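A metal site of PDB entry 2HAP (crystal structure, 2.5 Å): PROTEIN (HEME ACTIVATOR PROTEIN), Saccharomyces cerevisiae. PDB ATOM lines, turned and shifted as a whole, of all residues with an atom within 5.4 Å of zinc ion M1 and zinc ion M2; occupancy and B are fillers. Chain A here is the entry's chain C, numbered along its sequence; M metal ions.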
ATOM      1  N   ARG A   9      22.406 -11.082  19.714  1.00  0.00           N
ATOM      2  CA  ARG A   9      21.012 -10.672  19.837  1.00  0.00           C
ATOM      3  C   ARG A   9      20.407 -11.668  20.818  1.00  0.00           C
ATOM      4  O   ARG A   9      20.698 -12.864  20.712  1.00  0.00           O
ATOM      5  CB  ARG A   9      20.319 -10.795  18.489  1.00  0.00           C
ATOM      6  CG  ARG A   9      20.653 -12.060  17.751  1.00  0.00           C
ATOM      7  CD  ARG A   9      19.744 -12.231  16.558  1.00  0.00           C
ATOM      8  NE  ARG A   9      20.145 -13.373  15.763  1.00  0.00           N
ATOM      9  CZ  ARG A   9      19.416 -13.873  14.769  1.00  0.00           C
ATOM     10  NH1 ARG A   9      18.259 -13.307  14.465  1.00  0.00           N
ATOM     11  NH2 ARG A   9      19.831 -14.935  14.081  1.00  0.00           N
ATOM     12  N   CYS A  10      19.605 -11.200  21.779  1.00  0.00           N
ATOM     13  CA  CYS A  10      18.992 -12.101  22.758  1.00  0.00           C
ATOM     14  C   CYS A  10      18.277 -13.238  21.999  1.00  0.00           C
ATOM     15  O   CYS A  10      17.901 -13.103  20.820  1.00  0.00           O
ATOM     16  CB  CYS A  10      18.007 -11.351  23.663  1.00  0.00           C
ATOM     17  SG  CYS A  10      16.443 -11.075  22.807  1.00  0.00           S
ATOM     18  N   ILE A  12      15.310 -14.512  22.221  1.00  0.00           N
ATOM     19  CA  ILE A  12      13.938 -14.258  21.758  1.00  0.00           C
ATOM     20  C   ILE A  12      13.975 -13.517  20.426  1.00  0.00           C
ATOM     21  O   ILE A  12      13.196 -13.810  19.516  1.00  0.00           O
ATOM     22  CB  ILE A  12      13.137 -13.407  22.770  1.00  0.00           C
ATOM     23  CG1 ILE A  12      12.780 -14.255  23.979  1.00  0.00           C
ATOM     24  CG2 ILE A  12      11.846 -12.883  22.128  1.00  0.00           C
ATOM     25  CD1 ILE A  12      11.741 -15.309  23.697  1.00  0.00           C
ATOM     26  N   CYS A  13      14.901 -12.568  20.302  1.00  0.00           N
ATOM     27  CA  CYS A  13      14.999 -11.818  19.060  1.00  0.00           C
ATOM     28  C   CYS A  13      15.416 -12.720  17.898  1.00  0.00           C
ATOM     29  O   CYS A  13      14.922 -12.572  16.784  1.00  0.00           O
ATOM     30  CB  CYS A  13      15.971 -10.657  19.249  1.00  0.00           C
ATOM     31  SG  CYS A  13      15.161  -9.172  19.948  1.00  0.00           S
ATOM     32  N   LYS A  19      15.570  -7.268  15.205  1.00  0.00           N
ATOM     33  CA  LYS A  19      16.794  -6.603  15.660  1.00  0.00           C
ATOM     34  C   LYS A  19      16.842  -6.391  17.157  1.00  0.00           C
ATOM     35  O   LYS A  19      15.882  -5.903  17.748  1.00  0.00           O
ATOM     36  CB  LYS A  19      16.952  -5.232  14.994  1.00  0.00           C
ATOM     37  CG  LYS A  19      18.346  -4.955  14.458  1.00  0.00           C
ATOM     38  CD  LYS A  19      19.268  -4.289  15.478  1.00  0.00           C
ATOM     39  CE  LYS A  19      20.749  -4.504  15.095  1.00  0.00           C
ATOM     40  NZ  LYS A  19      21.708  -4.307  16.234  1.00  0.00           N
ATOM     41  N   CYS A  20      17.974  -6.765  17.754  1.00  0.00           N
ATOM     42  CA  CYS A  20      18.138  -6.625  19.184  1.00  0.00           C
ATOM     43  C   CYS A  20      19.042  -5.443  19.563  1.00  0.00           C
ATOM     44  O   CYS A  20      20.157  -5.336  19.073  1.00  0.00           O
ATOM     45  CB  CYS A  20      18.716  -7.928  19.734  1.00  0.00           C
ATOM     46  SG  CYS A  20      18.658  -8.051  21.549  1.00  0.00           S
ATOM     47  N   ASP A  21      18.553  -4.554  20.422  1.00  0.00           N
ATOM     48  CA  ASP A  21      19.377  -3.432  20.861  1.00  0.00           C
ATOM     49  C   ASP A  21      20.405  -3.934  21.869  1.00  0.00           C
ATOM     50  O   ASP A  21      21.055  -3.164  22.565  1.00  0.00           O
ATOM     51  CB  ASP A  21      18.534  -2.304  21.469  1.00  0.00           C
ATOM     52  CG  ASP A  21      17.636  -2.774  22.582  1.00  0.00           C
ATOM     53  OD1 ASP A  21      18.136  -3.488  23.486  1.00  0.00           O
ATOM     54  OD2 ASP A  21      16.436  -2.424  22.527  1.00  0.00           O
ATOM     55  N   HIS A  26      17.929  -6.963  29.901  1.00  0.00           N
ATOM     56  CA  HIS A  26      17.015  -7.436  28.876  1.00  0.00           C
ATOM     57  C   HIS A  26      16.911  -6.423  27.746  1.00  0.00           C
ATOM     58  O   HIS A  26      16.778  -5.239  27.993  1.00  0.00           O
ATOM     59  CB  HIS A  26      15.635  -7.694  29.464  1.00  0.00           C
ATOM     60  CG  HIS A  26      15.648  -8.439  30.776  1.00  0.00           C
ATOM     61  ND1 HIS A  26      16.221  -9.691  30.911  1.00  0.00           N
ATOM     62  CD2 HIS A  26      15.178  -8.096  31.990  1.00  0.00           C
ATOM     63  CE1 HIS A  26      16.102 -10.080  32.164  1.00  0.00           C
ATOM     64  NE2 HIS A  26      15.476  -9.137  32.837  1.00  0.00           N
ATOM     65  N   CYS A  27      16.956  -6.916  26.508  1.00  0.00           N
ATOM     66  CA  CYS A  27      16.840  -6.038  25.354  1.00  0.00           C
ATOM     67  C   CYS A  27      15.467  -5.368  25.404  1.00  0.00           C
ATOM     68  O   CYS A  27      14.505  -5.940  25.934  1.00  0.00           O
ATOM     69  CB  CYS A  27      17.009  -6.836  24.080  1.00  0.00           C
ATOM     70  SG  CYS A  27      15.484  -7.654  23.616  1.00  0.00           S
ATOM     71  N   GLN A  29      13.457  -4.815  22.929  1.00  0.00           N
ATOM     72  CA  GLN A  29      12.488  -5.402  22.017  1.00  0.00           C
ATOM     73  C   GLN A  29      11.593  -6.250  22.897  1.00  0.00           C
ATOM     74  O   GLN A  29      10.370  -6.112  22.865  1.00  0.00           O
ATOM     75  CB  GLN A  29      13.168  -6.274  20.968  1.00  0.00           C
ATOM     76  CG  GLN A  29      13.904  -5.496  19.892  1.00  0.00           C
ATOM     77  CD  GLN A  29      14.940  -4.490  20.442  1.00  0.00           C
ATOM     78  OE1 GLN A  29      15.788  -4.836  21.277  1.00  0.00           O
ATOM     79  NE2 GLN A  29      14.873  -3.258  19.975  1.00  0.00           N
ATOM     80  N   CYS A  30      12.207  -7.122  23.696  1.00  0.00           N
ATOM     81  CA  CYS A  30      11.467  -7.992  24.597  1.00  0.00           C
ATOM     82  C   CYS A  30      10.638  -7.185  25.594  1.00  0.00           C
ATOM     83  O   CYS A  30       9.469  -7.476  25.802  1.00  0.00           O
ATOM     84  CB  CYS A  30      12.414  -8.926  25.368  1.00  0.00           C
ATOM     85  SG  CYS A  30      13.093 -10.311  24.387  1.00  0.00           S
ATOM     86  N   CYS A  39      13.850 -12.902  28.176  1.00  0.00           N
ATOM     87  CA  CYS A  39      15.030 -12.418  27.449  1.00  0.00           C
ATOM     88  C   CYS A  39      16.256 -13.053  28.055  1.00  0.00           C
ATOM     89  O   CYS A  39      16.386 -13.126  29.279  1.00  0.00           O
ATOM     90  CB  CYS A  39      15.136 -10.877  27.575  1.00  0.00           C
ATOM     91  SG  CYS A  39      16.349 -10.066  26.459  1.00  0.00           S
ATOM     92  N   HIS A  40      17.176 -13.509  27.206  1.00  0.00           N
ATOM     93  CA  HIS A  40      18.403 -14.144  27.688  1.00  0.00           C
ATOM     94  C   HIS A  40      19.464 -14.122  26.582  1.00  0.00           C
ATOM     95  O   HIS A  40      19.154 -14.318  25.415  1.00  0.00           O
ATOM     96  CB  HIS A  40      18.097 -15.581  28.177  1.00  0.00           C
ATOM     97  CG  HIS A  40      19.144 -16.603  27.825  1.00  0.00           C
ATOM     98  ND1 HIS A  40      20.285 -16.791  28.576  1.00  0.00           N
ATOM     99  CD2 HIS A  40      19.223 -17.467  26.787  1.00  0.00           C
ATOM    100  CE1 HIS A  40      21.030 -17.723  28.014  1.00  0.00           C
ATOM    101  NE2 HIS A  40      20.420 -18.150  26.922  1.00  0.00           N
ATOM    102  N   TYR A  41      20.709 -13.852  26.954  1.00  0.00           N
ATOM    103  CA  TYR A  41      21.805 -13.844  25.992  1.00  0.00           C
ATOM    104  C   TYR A  41      22.679 -15.071  26.184  1.00  0.00           C
ATOM    105  O   TYR A  41      23.047 -15.400  27.314  1.00  0.00           O
ATOM    106  CB  TYR A  41      22.668 -12.565  26.151  1.00  0.00           C
ATOM    107  CG  TYR A  41      21.930 -11.275  25.852  1.00  0.00           C
ATOM    108  CD1 TYR A  41      21.693 -10.871  24.534  1.00  0.00           C
ATOM    109  CD2 TYR A  41      21.393 -10.497  26.882  1.00  0.00           C
ATOM    110  CE1 TYR A  41      20.961  -9.724  24.255  1.00  0.00           C
ATOM    111  CE2 TYR A  41      20.666  -9.358  26.613  1.00  0.00           C
ATOM    112  CZ  TYR A  41      20.436  -8.977  25.302  1.00  0.00           C
ATOM    113  OH  TYR A  41      19.655  -7.871  25.021  1.00  0.00           O
HETATM  114 ZN    ZN M   1      15.365  -9.891  24.416  1.00  0.00          ZN
HETATM  115 ZN    ZN M   2      16.369  -8.837  21.863  1.00  0.00          ZN
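The side-chain sulfur (SG) of Cys 10 sits close to the backbone NH (N) of Ile 12 (3.7 Å). SG of Cys 27 lies close to N of Gln 29 (3.6 Å). The backbone NH (N) of Cys 27 sits close to the side-chain hydroxyl (OH) of Tyr 41. The side-chain sulfur of Cys 20 lies close to the side-chain hydroxyl of Tyr 41.
Zinc ion M2 is bound by SG of Cys 13 (2.3 Å), SG of Cys 27 (2.3 Å), SG of Cys 10 (2.4 Å) and SG of Cys 20 (2.4 Å). Zinc ion M2 has four donor atoms within binding distance.
Zinc ion M1 is bound by SG of Cys 10 (2.3 Å), SG of Cys 39 (2.3 Å), SG of Cys 30 (2.3 Å) and SG of Cys 27 (2.4 Å). Zinc ion M1 has four donor atoms within binding distance.
Within 4 Å of zinc ion M2: Cys 10, Cys 13, Cys 20 and Cys 27.
Of the 14 residues printed, 4 come within 4 Å of zinc ion M1.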
